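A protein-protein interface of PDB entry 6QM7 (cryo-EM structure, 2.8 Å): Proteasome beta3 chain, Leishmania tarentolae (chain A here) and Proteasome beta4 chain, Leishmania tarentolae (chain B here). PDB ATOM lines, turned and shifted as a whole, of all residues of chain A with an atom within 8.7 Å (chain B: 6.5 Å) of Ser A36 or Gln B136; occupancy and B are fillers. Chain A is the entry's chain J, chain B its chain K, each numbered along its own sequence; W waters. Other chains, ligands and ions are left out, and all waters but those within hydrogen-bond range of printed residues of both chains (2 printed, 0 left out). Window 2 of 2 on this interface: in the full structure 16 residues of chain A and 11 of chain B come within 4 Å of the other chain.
Leu A28 touches Gln B136. CD1 of Ile A35 touches CE2 of Tyr B128, at 3.5 Å. CB of Ser A36 touches CG of Gln B136 (3.99 Å). Val A39 touches Gln B136 (CG2 to CD, 3.4 Å). CG of Arg A57 touches CG2 of Thr B134 (3.7 Å). Gln A61 touches Thr B134.
The side-chain carboxylate (OE2) of Glu A30 sits at hydrogen-bond distance from the side-chain hydroxyl (OH) of Tyr B128. OE1 of Gln A61 is in hydrogen-bond range of N of Leu B135 (2.7 Å).
Of the printed residues of chain B, Ser A36 touches Gln B136. Of the printed residues of chain A, Gln B136 touches Leu A28 (3.8 Å), Ser A36 (3.99 Å) and Val A39 (3.4 Å). Of the printed residues of chain A, Tyr B128 touches Glu A30 and Ile A35. Printed residues of chain A within 4 Å of Thr B134: Arg A57 and Gln A61. Of the printed residues of chain B, Arg A57 touches Thr B134. Of the printed residues of chain B, Val A39 touches Gln B136 (3.4 Å). Asn A26 touches none of the printed residues of chain B. The nearest printed residue of chain B that does not touch Glu A30 is Thr B134 (4.7 Å).
Water W2 bridges OG1 of Thr B134 (2.7 Å) and OG of Ser A7 (3.3 Å). Water W1 lies within hydrogen-bond range of O of Glu A38 (2.8 Å) and NE2 of Gln B136 (3.3 Å).
N of Val A39 sits at hydrogen-bond distance from O of Asn A26 (2.9 Å). The backbone carbonyl oxygen (O) of Leu A28 lies within hydrogen-bond range of the backbone NH (N) of Ile A35. O of Ser A36 lies within hydrogen-bond range of N of Leu A28 (2.9 Å). The side-chain hydroxyl (OG) of Ser A36 lies within hydrogen-bond range of the backbone NH (N) of Glu A38 (3.4 Å). The backbone carbonyl oxygen of Val A39 lies within hydrogen-bond range of the side-chain amino group of Lys A41 (3.1 Å). The backbone carbonyl oxygen (O) of Gln B136 lies within hydrogen-bond range of the backbone NH (N) of Tyr B128 (2.8 Å).
Of the 21 printed residues of chain A, 7 touch a printed residue of chain B. Printed residues of chain A that touch a printed residue of chain B: Leu A28, Glu A30, Ile A35, Ser A36, Val A39, Arg A57 and Gln A61. Along chain A the printed residues that touch a printed residue of chain B span positions 28 to 61. Of the 10 printed residues of chain B, 4 touch a printed residue of chain A. Hydrophobic or aromatic side chains of chain B within 4 Å of the printed part of chain A: Tyr B128 and Leu B135. Among the printed residues, no Asp or Glu carboxylate lies within 4 Å of a Lys or Arg side-chain nitrogen of the other chain.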
ATOM      1  N   SER A   7     -25.169  -1.105 -25.623  1.00  0.00           N
ATOM      2  CA  SER A   7     -24.804  -1.272 -24.196  1.00  0.00           C
ATOM      3  C   SER A   7     -24.924  -2.738 -23.799  1.00  0.00           C
ATOM      4  O   SER A   7     -24.340  -3.121 -22.775  1.00  0.00           O
ATOM      5  CB  SER A   7     -25.618  -0.371 -23.309  1.00  0.00           C
ATOM      6  OG  SER A   7     -25.222   0.978 -23.502  1.00  0.00           O
ATOM      7  N   ASP A  25     -29.412  -9.983 -16.816  1.00  0.00           N
ATOM      8  CA  ASP A  25     -27.964 -10.272 -16.872  1.00  0.00           C
ATOM      9  C   ASP A  25     -27.241  -9.127 -16.164  1.00  0.00           C
ATOM     10  O   ASP A  25     -27.921  -8.208 -15.703  1.00  0.00           O
ATOM     11  CB  ASP A  25     -27.493 -10.387 -18.319  1.00  0.00           C
ATOM     12  CG  ASP A  25     -27.343  -9.015 -18.938  1.00  0.00           C
ATOM     13  OD1 ASP A  25     -28.310  -8.219 -18.817  1.00  0.00           O
ATOM     14  OD2 ASP A  25     -26.252  -8.735 -19.487  1.00  0.00           O
ATOM     15  N   ASN A  26     -25.916  -9.157 -16.158  1.00  0.00           N
ATOM     16  CA  ASN A  26     -25.064  -8.222 -15.385  1.00  0.00           C
ATOM     17  C   ASN A  26     -24.106  -7.440 -16.287  1.00  0.00           C
ATOM     18  O   ASN A  26     -23.383  -6.591 -15.759  1.00  0.00           O
ATOM     19  CB  ASN A  26     -24.216  -8.996 -14.377  1.00  0.00           C
ATOM     20  CG  ASN A  26     -24.995  -9.510 -13.196  1.00  0.00           C
ATOM     21  OD1 ASN A  26     -24.985 -10.709 -12.916  1.00  0.00           O
ATOM     22  ND2 ASN A  26     -25.621  -8.591 -12.481  1.00  0.00           N
ATOM     23  N   ARG A  27     -24.042  -7.714 -17.580  1.00  0.00           N
ATOM     24  CA  ARG A  27     -23.010  -7.093 -18.441  1.00  0.00           C
ATOM     25  C   ARG A  27     -23.402  -5.669 -18.801  1.00  0.00           C
ATOM     26  O   ARG A  27     -24.563  -5.452 -19.131  1.00  0.00           O
ATOM     27  CB  ARG A  27     -22.866  -7.857 -19.748  1.00  0.00           C
ATOM     28  CG  ARG A  27     -21.612  -7.485 -20.519  1.00  0.00           C
ATOM     29  CD  ARG A  27     -21.597  -8.153 -21.872  1.00  0.00           C
ATOM     30  NE  ARG A  27     -20.610  -7.547 -22.738  1.00  0.00           N
ATOM     31  CZ  ARG A  27     -20.849  -6.595 -23.629  1.00  0.00           C
ATOM     32  NH1 ARG A  27     -22.067  -6.103 -23.796  1.00  0.00           N
ATOM     33  NH2 ARG A  27     -19.852  -6.147 -24.377  1.00  0.00           N
ATOM     34  N   LEU A  28     -22.443  -4.762 -18.787  1.00  0.00           N
ATOM     35  CA  LEU A  28     -22.555  -3.437 -19.441  1.00  0.00           C
ATOM     36  C   LEU A  28     -21.418  -3.332 -20.451  1.00  0.00           C
ATOM     37  O   LEU A  28     -20.277  -3.555 -20.052  1.00  0.00           O
ATOM     38  CB  LEU A  28     -22.445  -2.326 -18.394  1.00  0.00           C
ATOM     39  CG  LEU A  28     -22.319  -0.924 -18.988  1.00  0.00           C
ATOM     40  CD1 LEU A  28     -23.622  -0.529 -19.668  1.00  0.00           C
ATOM     41  CD2 LEU A  28     -21.911   0.115 -17.950  1.00  0.00           C
ATOM     42  N   GLY A  29     -21.719  -2.960 -21.688  1.00  0.00           N
ATOM     43  CA  GLY A  29     -20.725  -2.914 -22.769  1.00  0.00           C
ATOM     44  C   GLY A  29     -20.783  -1.630 -23.570  1.00  0.00           C
ATOM     45  O   GLY A  29     -21.618  -0.764 -23.276  1.00  0.00           O
ATOM     46  N   GLU A  30     -19.838  -1.490 -24.491  1.00  0.00           N
ATOM     47  CA  GLU A  30     -19.912  -0.596 -25.665  1.00  0.00           C
ATOM     48  C   GLU A  30     -19.595  -1.497 -26.853  1.00  0.00           C
ATOM     49  O   GLU A  30     -18.412  -1.814 -27.049  1.00  0.00           O
ATOM     50  CB  GLU A  30     -18.948   0.590 -25.567  1.00  0.00           C
ATOM     51  CG  GLU A  30     -18.642   1.023 -24.149  1.00  0.00           C
ATOM     52  CD  GLU A  30     -18.719   2.516 -23.874  1.00  0.00           C
ATOM     53  OE1 GLU A  30     -19.736   2.956 -23.249  1.00  0.00           O
ATOM     54  OE2 GLU A  30     -17.756   3.231 -24.249  1.00  0.00           O
ATOM     55  N   LYS A  33     -16.628  -4.414 -26.402  1.00  0.00           N
ATOM     56  CA  LYS A  33     -15.840  -4.176 -25.164  1.00  0.00           C
ATOM     57  C   LYS A  33     -16.808  -4.124 -23.983  1.00  0.00           C
ATOM     58  O   LYS A  33     -17.829  -3.451 -24.081  1.00  0.00           O
ATOM     59  CB  LYS A  33     -14.887  -2.976 -25.206  1.00  0.00           C
ATOM     60  CG  LYS A  33     -15.389  -1.644 -25.724  1.00  0.00           C
ATOM     61  CD  LYS A  33     -14.274  -0.603 -25.689  1.00  0.00           C
ATOM     62  CE  LYS A  33     -14.760   0.834 -25.614  1.00  0.00           C
ATOM     63  NZ  LYS A  33     -13.919   1.637 -24.693  1.00  0.00           N
ATOM     64  N   THR A  34     -16.482  -4.884 -22.946  1.00  0.00           N
ATOM     65  CA  THR A  34     -17.247  -5.054 -21.694  1.00  0.00           C
ATOM     66  C   THR A  34     -16.655  -4.101 -20.666  1.00  0.00           C
ATOM     67  O   THR A  34     -15.473  -4.267 -20.344  1.00  0.00           O
ATOM     68  CB  THR A  34     -17.142  -6.502 -21.213  1.00  0.00           C
ATOM     69  OG1 THR A  34     -17.746  -7.343 -22.202  1.00  0.00           O
ATOM     70  CG2 THR A  34     -17.765  -6.734 -19.857  1.00  0.00           C
ATOM     71  N   ILE A  35     -17.435  -3.132 -20.204  1.00  0.00           N
ATOM     72  CA  ILE A  35     -17.005  -2.116 -19.206  1.00  0.00           C
ATOM     73  C   ILE A  35     -17.134  -2.706 -17.814  1.00  0.00           C
ATOM     74  O   ILE A  35     -16.231  -2.480 -17.007  1.00  0.00           O
ATOM     75  CB  ILE A  35     -17.874  -0.860 -19.289  1.00  0.00           C
ATOM     76  CG1 ILE A  35     -17.782  -0.190 -20.658  1.00  0.00           C
ATOM     77  CG2 ILE A  35     -17.556   0.104 -18.156  1.00  0.00           C
ATOM     78  CD1 ILE A  35     -18.989   0.695 -20.913  1.00  0.00           C
ATOM     79  N   SER A  36     -18.272  -3.322 -17.514  1.00  0.00           N
ATOM     80  CA  SER A  36     -18.541  -3.891 -16.175  1.00  0.00           C
ATOM     81  C   SER A  36     -19.317  -5.188 -16.302  1.00  0.00           C
ATOM     82  O   SER A  36     -19.996  -5.377 -17.308  1.00  0.00           O
ATOM     83  CB  SER A  36     -19.253  -2.913 -15.293  1.00  0.00           C
ATOM     84  OG  SER A  36     -19.192  -3.315 -13.925  1.00  0.00           O
ATOM     85  N   THR A  37     -19.176  -6.033 -15.287  1.00  0.00           N
ATOM     86  CA  THR A  37     -19.811  -7.366 -15.164  1.00  0.00           C
ATOM     87  C   THR A  37     -20.717  -7.371 -13.937  1.00  0.00           C
ATOM     88  O   THR A  37     -21.132  -8.465 -13.533  1.00  0.00           O
ATOM     89  CB  THR A  37     -18.723  -8.440 -15.097  1.00  0.00           C
ATOM     90  OG1 THR A  37     -17.923  -8.216 -13.932  1.00  0.00           O
ATOM     91  CG2 THR A  37     -17.854  -8.443 -16.338  1.00  0.00           C
ATOM     92  N   GLU A  38     -20.990  -6.195 -13.374  1.00  0.00           N
ATOM     93  CA  GLU A  38     -21.759  -6.011 -12.120  1.00  0.00           C
ATOM     94  C   GLU A  38     -22.712  -4.834 -12.318  1.00  0.00           C
ATOM     95  O   GLU A  38     -22.701  -3.902 -11.497  1.00  0.00           O
ATOM     96  CB  GLU A  38     -20.794  -5.821 -10.950  1.00  0.00           C
ATOM     97  CG  GLU A  38     -20.273  -7.131 -10.382  1.00  0.00           C
ATOM     98  CD  GLU A  38     -18.862  -7.059  -9.813  1.00  0.00           C
ATOM     99  OE1 GLU A  38     -18.074  -8.007 -10.056  1.00  0.00           O
ATOM    100  OE2 GLU A  38     -18.549  -6.054  -9.126  1.00  0.00           O
ATOM    101  N   VAL A  39     -23.506  -4.891 -13.384  1.00  0.00           N
ATOM    102  CA  VAL A  39     -24.516  -3.861 -13.744  1.00  0.00           C
ATOM    103  C   VAL A  39     -25.819  -4.578 -14.013  1.00  0.00           C
ATOM    104  O   VAL A  39     -26.162  -4.806 -15.164  1.00  0.00           O
ATOM    105  CB  VAL A  39     -24.081  -3.036 -14.966  1.00  0.00           C
ATOM    106  CG1 VAL A  39     -25.067  -1.904 -15.287  1.00  0.00           C
ATOM    107  CG2 VAL A  39     -22.679  -2.485 -14.761  1.00  0.00           C
ATOM    108  N   PRO A  40     -26.576  -4.977 -12.974  1.00  0.00           N
ATOM    109  CA  PRO A  40     -27.896  -5.551 -13.186  1.00  0.00           C
ATOM    110  C   PRO A  40     -28.797  -4.412 -13.677  1.00  0.00           C
ATOM    111  O   PRO A  40     -28.511  -3.261 -13.391  1.00  0.00           O
ATOM    112  CB  PRO A  40     -28.336  -6.094 -11.824  1.00  0.00           C
ATOM    113  CG  PRO A  40     -27.150  -5.866 -10.897  1.00  0.00           C
ATOM    114  CD  PRO A  40     -26.253  -4.839 -11.554  1.00  0.00           C
ATOM    115  N   LYS A  41     -29.853  -4.758 -14.399  1.00  0.00           N
ATOM    116  CA  LYS A  41     -30.729  -3.776 -15.077  1.00  0.00           C
ATOM    117  C   LYS A  41     -32.099  -3.686 -14.390  1.00  0.00           C
ATOM    118  O   LYS A  41     -32.971  -3.033 -14.974  1.00  0.00           O
ATOM    119  CB  LYS A  41     -30.801  -4.171 -16.551  1.00  0.00           C
ATOM    120  CG  LYS A  41     -29.498  -3.929 -17.303  1.00  0.00           C
ATOM    121  CD  LYS A  41     -29.020  -5.108 -18.140  1.00  0.00           C
ATOM    122  CE  LYS A  41     -27.529  -5.358 -18.017  1.00  0.00           C
ATOM    123  NZ  LYS A  41     -26.756  -4.098 -18.133  1.00  0.00           N
ATOM    124  N   ARG A  57     -27.524   2.429 -22.568  1.00  0.00           N
ATOM    125  CA  ARG A  57     -27.346   2.490 -21.092  1.00  0.00           C
ATOM    126  C   ARG A  57     -27.663   3.889 -20.572  1.00  0.00           C
ATOM    127  O   ARG A  57     -28.307   3.976 -19.519  1.00  0.00           O
ATOM    128  CB  ARG A  57     -25.926   2.126 -20.649  1.00  0.00           C
ATOM    129  CG  ARG A  57     -25.690   2.187 -19.149  1.00  0.00           C
ATOM    130  CD  ARG A  57     -26.658   1.292 -18.418  1.00  0.00           C
ATOM    131  NE  ARG A  57     -26.506   1.419 -16.985  1.00  0.00           N
ATOM    132  CZ  ARG A  57     -27.344   0.913 -16.096  1.00  0.00           C
ATOM    133  NH1 ARG A  57     -28.416   0.239 -16.476  1.00  0.00           N
ATOM    134  NH2 ARG A  57     -27.108   1.089 -14.814  1.00  0.00           N
ATOM    135  N   GLN A  61     -30.489   4.791 -17.823  1.00  0.00           N
ATOM    136  CA  GLN A  61     -30.169   5.575 -16.605  1.00  0.00           C
ATOM    137  C   GLN A  61     -31.026   6.832 -16.544  1.00  0.00           C
ATOM    138  O   GLN A  61     -31.515   7.126 -15.445  1.00  0.00           O
ATOM    139  CB  GLN A  61     -28.692   5.932 -16.539  1.00  0.00           C
ATOM    140  CG  GLN A  61     -27.839   4.709 -16.280  1.00  0.00           C
ATOM    141  CD  GLN A  61     -26.408   5.085 -16.027  1.00  0.00           C
ATOM    142  OE1 GLN A  61     -25.714   5.568 -16.918  1.00  0.00           O
ATOM    143  NE2 GLN A  61     -25.962   4.847 -14.805  1.00  0.00           N
ATOM    144  N   LEU A 180     -23.448 -10.044 -26.165  1.00  0.00           N
ATOM    145  CA  LEU A 180     -23.701  -8.722 -25.538  1.00  0.00           C
ATOM    146  C   LEU A 180     -24.425  -8.852 -24.203  1.00  0.00           C
ATOM    147  O   LEU A 180     -24.744  -7.801 -23.657  1.00  0.00           O
ATOM    148  CB  LEU A 180     -24.538  -7.873 -26.505  1.00  0.00           C
ATOM    149  CG  LEU A 180     -23.794  -7.061 -27.567  1.00  0.00           C
ATOM    150  CD1 LEU A 180     -22.416  -7.628 -27.913  1.00  0.00           C
ATOM    151  CD2 LEU A 180     -24.652  -6.940 -28.820  1.00  0.00           C
ATOM    152  N   GLY A 182     -24.644 -11.381 -20.346  1.00  0.00           N
ATOM    153  CA  GLY A 182     -24.104 -12.452 -19.500  1.00  0.00           C
ATOM    154  C   GLY A 182     -23.448 -11.941 -18.232  1.00  0.00           C
ATOM    155  O   GLY A 182     -23.942 -10.984 -17.651  1.00  0.00           O
ATOM    156  N   TYR A 183     -22.367 -12.602 -17.830  1.00  0.00           N
ATOM    157  CA  TYR A 183     -21.707 -12.471 -16.512  1.00  0.00           C
ATOM    158  C   TYR A 183     -22.772 -12.736 -15.451  1.00  0.00           C
ATOM    159  O   TYR A 183     -22.959 -11.954 -14.504  1.00  0.00           O
ATOM    160  CB  TYR A 183     -20.955 -11.138 -16.437  1.00  0.00           C
ATOM    161  CG  TYR A 183     -19.979 -10.980 -17.572  1.00  0.00           C
ATOM    162  CD1 TYR A 183     -18.660 -11.372 -17.457  1.00  0.00           C
ATOM    163  CD2 TYR A 183     -20.415 -10.539 -18.808  1.00  0.00           C
ATOM    164  CE1 TYR A 183     -17.789 -11.274 -18.533  1.00  0.00           C
ATOM    165  CE2 TYR A 183     -19.561 -10.443 -19.892  1.00  0.00           C
ATOM    166  CZ  TYR A 183     -18.237 -10.801 -19.757  1.00  0.00           C
ATOM    167  OH  TYR A 183     -17.426 -10.663 -20.853  1.00  0.00           O
ATOM    168  N   LEU B 126     -14.632   6.023  -8.091  1.00  0.00           N
ATOM    169  CA  LEU B 126     -14.241   6.127  -9.506  1.00  0.00           C
ATOM    170  C   LEU B 126     -15.467   5.811 -10.344  1.00  0.00           C
ATOM    171  O   LEU B 126     -16.139   4.827 -10.036  1.00  0.00           O
ATOM    172  CB  LEU B 126     -13.106   5.150  -9.786  1.00  0.00           C
ATOM    173  CG  LEU B 126     -12.628   5.119 -11.231  1.00  0.00           C
ATOM    174  CD1 LEU B 126     -12.066   6.462 -11.667  1.00  0.00           C
ATOM    175  CD2 LEU B 126     -11.578   4.057 -11.406  1.00  0.00           C
ATOM    176  N   PHE B 127     -15.741   6.643 -11.336  1.00  0.00           N
ATOM    177  CA  PHE B 127     -16.929   6.555 -12.202  1.00  0.00           C
ATOM    178  C   PHE B 127     -16.491   6.658 -13.650  1.00  0.00           C
ATOM    179  O   PHE B 127     -15.962   7.695 -14.055  1.00  0.00           O
ATOM    180  CB  PHE B 127     -17.885   7.686 -11.864  1.00  0.00           C
ATOM    181  CG  PHE B 127     -18.542   7.506 -10.528  1.00  0.00           C
ATOM    182  CD1 PHE B 127     -19.684   6.739 -10.413  1.00  0.00           C
ATOM    183  CD2 PHE B 127     -17.993   8.079  -9.391  1.00  0.00           C
ATOM    184  CE1 PHE B 127     -20.278   6.561  -9.180  1.00  0.00           C
ATOM    185  CE2 PHE B 127     -18.594   7.914  -8.156  1.00  0.00           C
ATOM    186  CZ  PHE B 127     -19.735   7.151  -8.057  1.00  0.00           C
ATOM    187  N   TYR B 128     -16.697   5.590 -14.398  1.00  0.00           N
ATOM    188  CA  TYR B 128     -16.539   5.576 -15.869  1.00  0.00           C
ATOM    189  C   TYR B 128     -17.721   6.344 -16.447  1.00  0.00           C
ATOM    190  O   TYR B 128     -18.813   6.136 -15.928  1.00  0.00           O
ATOM    191  CB  TYR B 128     -16.420   4.123 -16.307  1.00  0.00           C
ATOM    192  CG  TYR B 128     -16.449   3.904 -17.790  1.00  0.00           C
ATOM    193  CD1 TYR B 128     -15.290   3.613 -18.495  1.00  0.00           C
ATOM    194  CD2 TYR B 128     -17.651   3.940 -18.477  1.00  0.00           C
ATOM    195  CE1 TYR B 128     -15.320   3.387 -19.861  1.00  0.00           C
ATOM    196  CE2 TYR B 128     -17.693   3.746 -19.845  1.00  0.00           C
ATOM    197  CZ  TYR B 128     -16.529   3.454 -20.537  1.00  0.00           C
ATOM    198  OH  TYR B 128     -16.592   3.249 -21.885  1.00  0.00           O
ATOM    199  N   MET B 129     -17.512   7.241 -17.412  1.00  0.00           N
ATOM    200  CA  MET B 129     -18.627   7.943 -18.106  1.00  0.00           C
ATOM    201  C   MET B 129     -18.340   8.004 -19.596  1.00  0.00           C
ATOM    202  O   MET B 129     -17.301   8.522 -19.965  1.00  0.00           O
ATOM    203  CB  MET B 129     -18.895   9.359 -17.591  1.00  0.00           C
ATOM    204  CG  MET B 129     -18.465   9.574 -16.144  1.00  0.00           C
ATOM    205  SD  MET B 129     -19.242  10.924 -15.189  1.00  0.00           S
ATOM    206  CE  MET B 129     -20.298  11.649 -16.442  1.00  0.00           C
ATOM    207  N   THR B 134     -23.598   7.550 -20.111  1.00  0.00           N
ATOM    208  CA  THR B 134     -23.432   6.267 -19.399  1.00  0.00           C
ATOM    209  C   THR B 134     -22.567   6.512 -18.166  1.00  0.00           C
ATOM    210  O   THR B 134     -21.401   6.807 -18.362  1.00  0.00           O
ATOM    211  CB  THR B 134     -22.724   5.258 -20.306  1.00  0.00           C
ATOM    212  OG1 THR B 134     -23.477   5.122 -21.517  1.00  0.00           O
ATOM    213  CG2 THR B 134     -22.505   3.929 -19.615  1.00  0.00           C
ATOM    214  N   LEU B 135     -23.113   6.424 -16.962  1.00  0.00           N
ATOM    215  CA  LEU B 135     -22.333   6.457 -15.701  1.00  0.00           C
ATOM    216  C   LEU B 135     -22.233   5.039 -15.146  1.00  0.00           C
ATOM    217  O   LEU B 135     -23.263   4.349 -15.101  1.00  0.00           O
ATOM    218  CB  LEU B 135     -23.066   7.376 -14.721  1.00  0.00           C
ATOM    219  CG  LEU B 135     -22.391   7.607 -13.375  1.00  0.00           C
ATOM    220  CD1 LEU B 135     -21.051   8.285 -13.580  1.00  0.00           C
ATOM    221  CD2 LEU B 135     -23.273   8.454 -12.466  1.00  0.00           C
ATOM    222  N   GLN B 136     -21.051   4.612 -14.728  1.00  0.00           N
ATOM    223  CA  GLN B 136     -20.869   3.307 -14.041  1.00  0.00           C
ATOM    224  C   GLN B 136     -19.759   3.429 -13.013  1.00  0.00           C
ATOM    225  O   GLN B 136     -18.661   3.836 -13.388  1.00  0.00           O
ATOM    226  CB  GLN B 136     -20.510   2.193 -15.027  1.00  0.00           C
ATOM    227  CG  GLN B 136     -20.509   0.774 -14.447  1.00  0.00           C
ATOM    228  CD  GLN B 136     -21.593   0.477 -13.436  1.00  0.00           C
ATOM    229  OE1 GLN B 136     -22.771   0.763 -13.655  1.00  0.00           O
ATOM    230  NE2 GLN B 136     -21.207  -0.102 -12.311  1.00  0.00           N
ATOM    231  N   ALA B 137     -20.040   3.086 -11.767  1.00  0.00           N
ATOM    232  CA  ALA B 137     -18.974   2.918 -10.768  1.00  0.00           C
ATOM    233  C   ALA B 137     -18.106   1.756 -11.242  1.00  0.00           C
ATOM    234  O   ALA B 137     -18.665   0.743 -11.705  1.00  0.00           O
ATOM    235  CB  ALA B 137     -19.538   2.682  -9.393  1.00  0.00           C
ATOM    236  N   VAL B 138     -16.791   1.916 -11.164  1.00  0.00           N
ATOM    237  CA  VAL B 138     -15.826   0.854 -11.541  1.00  0.00           C
ATOM    238  C   VAL B 138     -14.650   0.910 -10.582  1.00  0.00           C
ATOM    239  O   VAL B 138     -14.352   1.962 -10.034  1.00  0.00           O
ATOM    240  CB  VAL B 138     -15.350   1.011 -12.992  1.00  0.00           C
ATOM    241  CG1 VAL B 138     -16.500   0.890 -13.987  1.00  0.00           C
ATOM    242  CG2 VAL B 138     -14.566   2.299 -13.206  1.00  0.00           C
ATOM    243  N   PRO B 139     -13.948  -0.220 -10.368  1.00  0.00           N
ATOM    244  CA  PRO B 139     -12.695  -0.218  -9.621  1.00  0.00           C
ATOM    245  C   PRO B 139     -11.556   0.370 -10.455  1.00  0.00           C
ATOM    246  O   PRO B 139     -10.611   0.838  -9.905  1.00  0.00           O
ATOM    247  CB  PRO B 139     -12.478  -1.702  -9.341  1.00  0.00           C
ATOM    248  CG  PRO B 139     -13.062  -2.350 -10.557  1.00  0.00           C
ATOM    249  CD  PRO B 139     -14.309  -1.552 -10.856  1.00  0.00           C
HETATM  250  O   HOH W   1     -23.483  -1.434 -10.346  1.00  0.00           O
HETATM  251  O   HOH W   2     -24.676   4.273 -23.736  1.00  0.00           O
